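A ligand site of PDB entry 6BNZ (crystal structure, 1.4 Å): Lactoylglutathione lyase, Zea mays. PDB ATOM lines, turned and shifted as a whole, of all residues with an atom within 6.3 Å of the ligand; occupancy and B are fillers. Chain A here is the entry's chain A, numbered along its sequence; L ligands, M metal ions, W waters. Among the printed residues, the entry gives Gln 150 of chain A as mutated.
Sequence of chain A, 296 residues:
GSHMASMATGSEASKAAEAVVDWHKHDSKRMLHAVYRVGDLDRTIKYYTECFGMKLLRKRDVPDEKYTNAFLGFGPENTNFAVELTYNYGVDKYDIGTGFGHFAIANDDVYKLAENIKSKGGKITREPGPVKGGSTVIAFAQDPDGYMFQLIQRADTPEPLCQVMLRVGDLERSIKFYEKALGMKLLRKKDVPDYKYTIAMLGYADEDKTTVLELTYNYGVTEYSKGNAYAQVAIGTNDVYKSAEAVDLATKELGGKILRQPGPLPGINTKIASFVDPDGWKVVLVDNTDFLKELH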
ATOM      1  N   GLY A 101      17.746   3.943  -8.411  1.00  0.00           N
ATOM      2  CA  GLY A 101      17.573   2.852  -9.372  1.00  0.00           C
ATOM      3  C   GLY A 101      18.372   1.603  -9.053  1.00  0.00           C
ATOM      4  O   GLY A 101      17.791   0.594  -8.594  1.00  0.00           O
ATOM      5  N   HIS A 102      19.657   1.649  -9.419  1.00  0.00           N
ATOM      6  CA  HIS A 102      20.547   0.461  -9.198  1.00  0.00           C
ATOM      7  C   HIS A 102      22.015   0.843  -9.326  1.00  0.00           C
ATOM      8  O   HIS A 102      22.347   1.947  -9.827  1.00  0.00           O
ATOM      9  CB  HIS A 102      20.257  -0.640 -10.218  1.00  0.00           C
ATOM     10  CG  HIS A 102      20.357  -0.229 -11.669  1.00  0.00           C
ATOM     11  ND1 HIS A 102      19.242  -0.071 -12.471  1.00  0.00           N
ATOM     12  CD2 HIS A 102      21.432  -0.022 -12.475  1.00  0.00           C
ATOM     13  CE1 HIS A 102      19.624   0.236 -13.688  1.00  0.00           C
ATOM     14  NE2 HIS A 102      20.952   0.287 -13.730  1.00  0.00           N
ATOM     15  N   ARG A 126      15.672 -10.938 -11.659  1.00  0.00           N
ATOM     16  CA  ARG A 126      15.445 -10.854 -13.080  1.00  0.00           C
ATOM     17  C   ARG A 126      16.493 -11.730 -13.674  1.00  0.00           C
ATOM     18  O   ARG A 126      17.695 -11.436 -13.665  1.00  0.00           O
ATOM     19  CB  ARG A 126      15.495  -9.392 -13.574  1.00  0.00           C
ATOM     20  CG  ARG A 126      14.844  -9.103 -14.918  1.00  0.00           C
ATOM     21  CD  ARG A 126      15.706  -9.534 -16.099  1.00  0.00           C
ATOM     22  NE  ARG A 126      15.366  -8.936 -17.383  1.00  0.00           N
ATOM     23  CZ  ARG A 126      16.013  -9.173 -18.506  1.00  0.00           C
ATOM     24  NH1 ARG A 126      17.044 -10.050 -18.546  1.00  0.00           N
ATOM     25  NH2 ARG A 126      15.615  -8.573 -19.635  1.00  0.00           N
ATOM     26  N   PRO A 130      18.442 -11.062 -22.812  1.00  0.00           N
ATOM     27  CA  PRO A 130      18.462  -9.711 -23.454  1.00  0.00           C
ATOM     28  C   PRO A 130      17.497  -8.741 -22.798  1.00  0.00           C
ATOM     29  O   PRO A 130      16.443  -9.154 -22.293  1.00  0.00           O
ATOM     30  CB  PRO A 130      18.043 -10.004 -24.917  1.00  0.00           C
ATOM     31  CG  PRO A 130      17.316 -11.300 -24.808  1.00  0.00           C
ATOM     32  CD  PRO A 130      18.101 -12.092 -23.798  1.00  0.00           C
ATOM     33  N   VAL A 131      17.873  -7.466 -22.794  1.00  0.00           N
ATOM     34  CA  VAL A 131      17.005  -6.426 -22.245  1.00  0.00           C
ATOM     35  C   VAL A 131      15.704  -6.394 -23.106  1.00  0.00           C
ATOM     36  O   VAL A 131      15.760  -6.626 -24.321  1.00  0.00           O
ATOM     37  CB  VAL A 131      17.746  -5.063 -22.097  1.00  0.00           C
ATOM     38  CG1 VAL A 131      18.279  -4.553 -23.425  1.00  0.00           C
ATOM     39  CG2 VAL A 131      16.851  -4.011 -21.418  1.00  0.00           C
ATOM     40  N   LYS A 132      14.560  -6.192 -22.440  1.00  0.00           N
ATOM     41  CA  LYS A 132      13.254  -6.159 -23.136  1.00  0.00           C
ATOM     42  C   LYS A 132      13.198  -5.064 -24.205  1.00  0.00           C
ATOM     43  O   LYS A 132      13.192  -3.859 -23.886  1.00  0.00           O
ATOM     44  CB  LYS A 132      12.096  -6.044 -22.128  1.00  0.00           C
ATOM     45  CG  LYS A 132      11.333  -7.334 -21.962  1.00  0.00           C
ATOM     46  CD  LYS A 132      10.806  -7.484 -20.553  1.00  0.00           C
ATOM     47  CE  LYS A 132      10.644  -8.963 -20.227  1.00  0.00           C
ATOM     48  NZ  LYS A 132      11.329  -9.272 -18.943  1.00  0.00           N
ATOM     49  N   ILE A 138      21.339  -8.827 -19.751  1.00  0.00           N
ATOM     50  CA  ILE A 138      21.311  -8.245 -18.421  1.00  0.00           C
ATOM     51  C   ILE A 138      20.678  -9.228 -17.447  1.00  0.00           C
ATOM     52  O   ILE A 138      19.987 -10.198 -17.889  1.00  0.00           O
ATOM     53  CB  ILE A 138      20.577  -6.870 -18.377  1.00  0.00           C
ATOM     54  CG1 ILE A 138      19.070  -6.982 -18.771  1.00  0.00           C
ATOM     55  CG2 ILE A 138      21.302  -5.830 -19.255  1.00  0.00           C
ATOM     56  CD1 ILE A 138      18.280  -5.811 -18.224  1.00  0.00           C
ATOM     57  N   PHE A 140      19.194  -8.954 -12.920  1.00  0.00           N
ATOM     58  CA  PHE A 140      19.170  -8.132 -11.694  1.00  0.00           C
ATOM     59  C   PHE A 140      19.288  -8.969 -10.437  1.00  0.00           C
ATOM     60  O   PHE A 140      18.647 -10.062 -10.332  1.00  0.00           O
ATOM     61  CB  PHE A 140      17.893  -7.273 -11.579  1.00  0.00           C
ATOM     62  CG  PHE A 140      17.892  -6.006 -12.394  1.00  0.00           C
ATOM     63  CD1 PHE A 140      18.414  -4.858 -11.841  1.00  0.00           C
ATOM     64  CD2 PHE A 140      17.368  -5.966 -13.691  1.00  0.00           C
ATOM     65  CE1 PHE A 140      18.428  -3.661 -12.575  1.00  0.00           C
ATOM     66  CE2 PHE A 140      17.346  -4.772 -14.428  1.00  0.00           C
ATOM     67  CZ  PHE A 140      17.900  -3.617 -13.859  1.00  0.00           C
ATOM     68  N   GLN A 150      22.154  -4.226 -11.269  1.00  0.00           N
ATOM     69  CA  GLN A 150      22.034  -4.771 -12.592  1.00  0.00           C
ATOM     70  C   GLN A 150      23.360  -5.471 -12.931  1.00  0.00           C
ATOM     71  O   GLN A 150      24.451  -4.946 -12.653  1.00  0.00           O
ATOM     72  CB  GLN A 150      21.792  -3.637 -13.580  1.00  0.00           C
ATOM     73  CG  GLN A 150      21.473  -4.096 -14.997  1.00  0.00           C
ATOM     74  CD  GLN A 150      21.139  -2.950 -15.925  1.00  0.00           C
ATOM     75  OE1 GLN A 150      21.712  -1.859 -15.811  1.00  0.00           O
ATOM     76  NE2 GLN A 150      20.303  -3.219 -16.915  1.00  0.00           N
ATOM     77  N   MET A 165      22.451   4.251 -11.290  1.00  0.00           N
ATOM     78  CA  MET A 165      21.234   4.718 -12.019  1.00  0.00           C
ATOM     79  C   MET A 165      20.294   5.357 -11.021  1.00  0.00           C
ATOM     80  O   MET A 165      19.939   4.768  -9.960  1.00  0.00           O
ATOM     81  CB  MET A 165      20.518   3.518 -12.664  1.00  0.00           C
ATOM     82  CG  MET A 165      19.359   3.952 -13.608  1.00  0.00           C
ATOM     83  SD  MET A 165      17.788   4.398 -12.809  1.00  0.00           S
ATOM     84  CE  MET A 165      16.981   2.761 -12.902  1.00  0.00           C
ATOM     85  N   ARG A 167      16.547   7.870 -10.827  1.00  0.00           N
ATOM     86  CA  ARG A 167      15.345   8.324 -11.570  1.00  0.00           C
ATOM     87  C   ARG A 167      15.267   9.854 -11.439  1.00  0.00           C
ATOM     88  O   ARG A 167      15.505  10.416 -10.386  1.00  0.00           O
ATOM     89  CB  ARG A 167      14.083   7.603 -11.051  1.00  0.00           C
ATOM     90  CG  ARG A 167      14.193   6.092 -11.323  1.00  0.00           C
ATOM     91  CD  ARG A 167      12.947   5.368 -10.797  1.00  0.00           C
ATOM     92  NE  ARG A 167      13.169   3.940 -11.072  1.00  0.00           N
ATOM     93  CZ  ARG A 167      13.721   3.084 -10.220  1.00  0.00           C
ATOM     94  NH1 ARG A 167      13.880   3.412  -8.956  1.00  0.00           N
ATOM     95  NH2 ARG A 167      14.018   1.869 -10.676  1.00  0.00           N
ATOM     96  N   VAL A 192      12.346   4.472 -24.939  1.00  0.00           N
ATOM     97  CA  VAL A 192      11.814   3.110 -24.993  1.00  0.00           C
ATOM     98  C   VAL A 192      10.276   3.242 -24.848  1.00  0.00           C
ATOM     99  O   VAL A 192       9.699   2.949 -23.798  1.00  0.00           O
ATOM    100  CB  VAL A 192      12.461   2.197 -23.925  1.00  0.00           C
ATOM    101  CG1 VAL A 192      12.032   0.737 -24.121  1.00  0.00           C
ATOM    102  CG2 VAL A 192      14.002   2.253 -24.002  1.00  0.00           C
ATOM    103  N   TYR A 195       7.755   0.686 -23.335  1.00  0.00           N
ATOM    104  CA  TYR A 195       7.744   0.527 -21.884  1.00  0.00           C
ATOM    105  C   TYR A 195       7.734   1.867 -21.142  1.00  0.00           C
ATOM    106  O   TYR A 195       7.873   1.899 -19.940  1.00  0.00           O
ATOM    107  CB  TYR A 195       8.914  -0.360 -21.441  1.00  0.00           C
ATOM    108  CG  TYR A 195       8.829  -1.711 -22.052  1.00  0.00           C
ATOM    109  CD1 TYR A 195       7.826  -2.595 -21.651  1.00  0.00           C
ATOM    110  CD2 TYR A 195       9.645  -2.046 -23.110  1.00  0.00           C
ATOM    111  CE1 TYR A 195       7.722  -3.852 -22.250  1.00  0.00           C
ATOM    112  CE2 TYR A 195       9.562  -3.311 -23.715  1.00  0.00           C
ATOM    113  CZ  TYR A 195       8.592  -4.188 -23.298  1.00  0.00           C
ATOM    114  OH  TYR A 195       8.498  -5.431 -23.899  1.00  0.00           O
ATOM    115  N   LYS A 196       7.438   2.927 -21.854  1.00  0.00           N
ATOM    116  CA  LYS A 196       7.191   4.275 -21.331  1.00  0.00           C
ATOM    117  C   LYS A 196       8.317   4.825 -20.412  1.00  0.00           C
ATOM    118  O   LYS A 196       8.043   5.369 -19.318  1.00  0.00           O
ATOM    119  CB  LYS A 196       5.847   4.320 -20.613  1.00  0.00           C
ATOM    120  CG  LYS A 196       4.737   3.844 -21.581  1.00  0.00           C
ATOM    121  CD  LYS A 196       3.381   4.285 -21.067  1.00  0.00           C
ATOM    122  CE  LYS A 196       2.338   3.267 -21.513  1.00  0.00           C
ATOM    123  NZ  LYS A 196       1.434   2.985 -20.347  1.00  0.00           N
ATOM    124  N   TYR A 197       9.524   4.672 -20.932  1.00  0.00           N
ATOM    125  CA  TYR A 197      10.686   5.268 -20.244  1.00  0.00           C
ATOM    126  C   TYR A 197      11.708   5.755 -21.245  1.00  0.00           C
ATOM    127  O   TYR A 197      11.690   5.363 -22.451  1.00  0.00           O
ATOM    128  CB  TYR A 197      11.279   4.342 -19.189  1.00  0.00           C
ATOM    129  CG  TYR A 197      12.087   3.159 -19.725  1.00  0.00           C
ATOM    130  CD1 TYR A 197      13.456   3.254 -20.026  1.00  0.00           C
ATOM    131  CD2 TYR A 197      11.467   1.917 -19.921  1.00  0.00           C
ATOM    132  CE1 TYR A 197      14.190   2.182 -20.528  1.00  0.00           C
ATOM    133  CE2 TYR A 197      12.189   0.854 -20.422  1.00  0.00           C
ATOM    134  CZ  TYR A 197      13.544   0.976 -20.707  1.00  0.00           C
ATOM    135  OH  TYR A 197      14.265  -0.102 -21.211  1.00  0.00           O
ATOM    136  N   ILE A 199      16.068   6.775 -21.203  1.00  0.00           N
ATOM    137  CA  ILE A 199      17.309   6.820 -20.360  1.00  0.00           C
ATOM    138  C   ILE A 199      18.366   7.702 -20.982  1.00  0.00           C
ATOM    139  O   ILE A 199      18.384   7.941 -22.167  1.00  0.00           O
ATOM    140  CB  ILE A 199      17.924   5.412 -20.119  1.00  0.00           C
ATOM    141  CG1 ILE A 199      18.353   4.715 -21.427  1.00  0.00           C
ATOM    142  CG2 ILE A 199      16.960   4.558 -19.342  1.00  0.00           C
ATOM    143  CD1 ILE A 199      19.858   4.948 -21.730  1.00  0.00           C
ATOM    144  N   GLU A 214      23.552   6.848 -15.027  1.00  0.00           N
ATOM    145  CA  GLU A 214      22.373   6.531 -15.890  1.00  0.00           C
ATOM    146  C   GLU A 214      21.194   7.211 -15.229  1.00  0.00           C
ATOM    147  O   GLU A 214      20.908   7.012 -14.023  1.00  0.00           O
ATOM    148  CB  GLU A 214      22.087   5.026 -15.947  1.00  0.00           C
ATOM    149  CG  GLU A 214      20.960   4.611 -16.920  1.00  0.00           C
ATOM    150  CD  GLU A 214      20.616   3.133 -16.840  1.00  0.00           C
ATOM    151  OE1 GLU A 214      21.243   2.375 -16.073  1.00  0.00           O
ATOM    152  OE2 GLU A 214      19.654   2.725 -17.521  1.00  0.00           O
ATOM    153  N   THR A 216      17.090   7.848 -15.494  1.00  0.00           N
ATOM    154  CA  THR A 216      15.861   7.259 -16.081  1.00  0.00           C
ATOM    155  C   THR A 216      14.639   8.167 -15.814  1.00  0.00           C
ATOM    156  O   THR A 216      14.348   8.601 -14.673  1.00  0.00           O
ATOM    157  CB  THR A 216      15.566   5.867 -15.411  1.00  0.00           C
ATOM    158  OG1 THR A 216      16.661   5.007 -15.731  1.00  0.00           O
ATOM    159  CG2 THR A 216      14.267   5.228 -15.961  1.00  0.00           C
ATOM    160  N   TYR A 217      13.909   8.446 -16.901  1.00  0.00           N
ATOM    161  CA  TYR A 217      12.642   9.165 -16.814  1.00  0.00           C
ATOM    162  C   TYR A 217      11.524   8.157 -17.170  1.00  0.00           C
ATOM    163  O   TYR A 217      11.661   7.444 -18.186  1.00  0.00           O
ATOM    164  CB  TYR A 217      12.701  10.308 -17.863  1.00  0.00           C
ATOM    165  CG  TYR A 217      11.334  10.912 -18.139  1.00  0.00           C
ATOM    166  CD1 TYR A 217      10.728  11.759 -17.199  1.00  0.00           C
ATOM    167  CD2 TYR A 217      10.704  10.632 -19.350  1.00  0.00           C
ATOM    168  CE1 TYR A 217       9.437  12.308 -17.427  1.00  0.00           C
ATOM    169  CE2 TYR A 217       9.435  11.212 -19.599  1.00  0.00           C
ATOM    170  CZ  TYR A 217       8.813  11.953 -18.629  1.00  0.00           C
ATOM    171  OH  TYR A 217       7.553  12.553 -18.844  1.00  0.00           O
ATOM    172  N   ASN A 218      10.473   8.124 -16.337  1.00  0.00           N
ATOM    173  CA  ASN A 218       9.236   7.307 -16.634  1.00  0.00           C
ATOM    174  C   ASN A 218       8.150   8.292 -17.032  1.00  0.00           C
ATOM    175  O   ASN A 218       7.982   9.322 -16.426  1.00  0.00           O
ATOM    176  CB  ASN A 218       8.842   6.572 -15.352  1.00  0.00           C
ATOM    177  CG  ASN A 218       9.762   5.418 -15.062  1.00  0.00           C
ATOM    178  OD1 ASN A 218       9.727   4.417 -15.733  1.00  0.00           O
ATOM    179  ND2 ASN A 218      10.613   5.548 -14.011  1.00  0.00           N
ATOM    180  N   TYR A 224      10.086  11.689  -7.189  1.00  0.00           N
ATOM    181  CA  TYR A 224      10.400  10.418  -6.513  1.00  0.00           C
ATOM    182  C   TYR A 224      10.911  10.699  -5.110  1.00  0.00           C
ATOM    183  O   TYR A 224      11.408  11.824  -4.813  1.00  0.00           O
ATOM    184  CB  TYR A 224      11.537   9.710  -7.225  1.00  0.00           C
ATOM    185  CG  TYR A 224      11.203   9.310  -8.607  1.00  0.00           C
ATOM    186  CD1 TYR A 224      11.451  10.187  -9.701  1.00  0.00           C
ATOM    187  CD2 TYR A 224      10.657   8.057  -8.894  1.00  0.00           C
ATOM    188  CE1 TYR A 224      11.154   9.795 -11.002  1.00  0.00           C
ATOM    189  CE2 TYR A 224      10.353   7.658 -10.227  1.00  0.00           C
ATOM    190  CZ  TYR A 224      10.611   8.508 -11.266  1.00  0.00           C
ATOM    191  OH  TYR A 224      10.357   8.188 -12.590  1.00  0.00           O
HETATM  192  N1  LIG L   1      10.362   1.821 -14.989  1.00  0.00           N
HETATM  193  C1  LIG L   1      11.767   1.423 -15.111  1.00  0.00           C
HETATM  194  C2  LIG L   1      12.551   2.038 -13.983  1.00  0.00           C
HETATM  195  O1  LIG L   1      13.485   1.370 -13.420  1.00  0.00           O
HETATM  196  O2  LIG L   1      12.176   3.165 -13.582  1.00  0.00           O
HETATM  197  C3  LIG L   1      12.229   1.982 -16.459  1.00  0.00           C
HETATM  198  C4  LIG L   1      13.671   1.606 -16.810  1.00  0.00           C
HETATM  199  C5  LIG L   1      13.872   0.209 -17.353  1.00  0.00           C
HETATM  200  O3  LIG L   1      12.921  -0.586 -17.426  1.00  0.00           O
HETATM  201  N2  LIG L   1      15.170  -0.062 -17.707  1.00  0.00           N
HETATM  202  C6  LIG L   1      15.543  -1.369 -18.252  1.00  0.00           C
HETATM  203  C7  LIG L   1      15.018  -2.486 -17.355  1.00  0.00           C
HETATM  204  O4  LIG L   1      15.189  -2.457 -16.158  1.00  0.00           O
HETATM  205  C8  LIG L   1      17.042  -1.512 -18.597  1.00  0.00           C
HETATM  206  S1  LIG L   1      17.597  -0.072 -19.590  1.00  0.00           S
HETATM  207  N3  LIG L   1      14.314  -3.420 -17.992  1.00  0.00           N
HETATM  208  C9  LIG L   1      13.720  -4.570 -17.345  1.00  0.00           C
HETATM  209  C10 LIG L   1      13.926  -5.879 -18.129  1.00  0.00           C
HETATM  210  O5  LIG L   1      14.528  -5.881 -19.244  1.00  0.00           O
HETATM  211  O6  LIG L   1      13.488  -6.919 -17.570  1.00  0.00           O
HETATM  212 CO    CO M   1      21.461   0.262 -15.834  1.00  0.00          CO
HETATM  213  O   HOH W   1      13.291  -2.598 -21.181  1.00  0.00           O
HETATM  214  O   HOH W   2       8.733   0.467 -17.080  1.00  0.00           O
HETATM  215  O   HOH W   3      17.011   2.275 -16.572  1.00  0.00           O
HETATM  216  O   HOH W   4      10.571  -1.550 -17.754  1.00  0.00           O
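Water W2 lies within hydrogen-bond range of a nitrogen (N1) of the ligand (3.0 Å) and the backbone carbonyl oxygen of Tyr 195 (3.3 Å). Water W3 lies within hydrogen-bond range of the side-chain carboxylate of Glu 214 (2.8 Å), the side-chain hydroxyl of Thr 216 (2.9 Å) and a nitrogen (N2) of the ligand (3.2 Å). Water W1 lies within hydrogen-bond range of OH of Tyr 197 (2.7 Å), O of Lys 132 (3.0 Å) and N3 of the ligand (3.4 Å).
The backbone carbonyl oxygen of Arg 126 lies within hydrogen-bond range of the backbone NH of Phe 140. NH1 of Arg 126 lies within hydrogen-bond range of O of Ile 138, at 3.0 Å. The guanidinium group (NH2) of Arg 126 is in hydrogen-bond range of the backbone carbonyl oxygen (O) of Pro 130, at 2.8 Å. The side-chain hydroxyl of Tyr 224 is in hydrogen-bond range of the side-chain amide nitrogen of Asn 218 (3.0 Å). The backbone carbonyl oxygen (O) of Tyr 197 sits at hydrogen-bond distance from the backbone NH (N) of Val 192. The side-chain hydroxyl (OG1) of Thr 216 is in hydrogen-bond range of the side-chain sulfur (SD) of Met 165 (3.2 Å). The backbone carbonyl oxygen (O) of His 102 lies within hydrogen-bond range of the backbone NH (N) of Met 165, at 2.7 Å. The backbone carbonyl oxygen of Met 165 is in hydrogen-bond range of the backbone NH of Gly 101 (2.8 Å).
Residues that only touch the ligand: Val 131 (3.7 Å), Ile 138 (3.9 Å), Phe 140 (3.6 Å), Met 165 (3.8 Å) and Thr 216 (3.8 Å). Hydrophobic or aromatic side chains within 4 Å of the ligand: Val 131, Ile 138, Phe 140, Met 165 and Tyr 197. Of the 21 residues printed, 10 come within 4 Å of the ligand.
NE of Arg 126 is in salt-bridge range of O6 of the ligand (2.8 Å). N1 of the ligand sits at hydrogen-bond distance from OD1 of Asn 218, 2.8 Å away. NE of Arg 167 is in salt-bridge range of O2 of the ligand (2.8 Å). The backbone NH (N) of Lys 132 is in hydrogen-bond range of an oxygen (O5) of the ligand (3.2 Å). NZ of Lys 132 is in salt-bridge range of O6 of the ligand (3.5 Å). OH of Tyr 197 sits close to S1 of the ligand.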
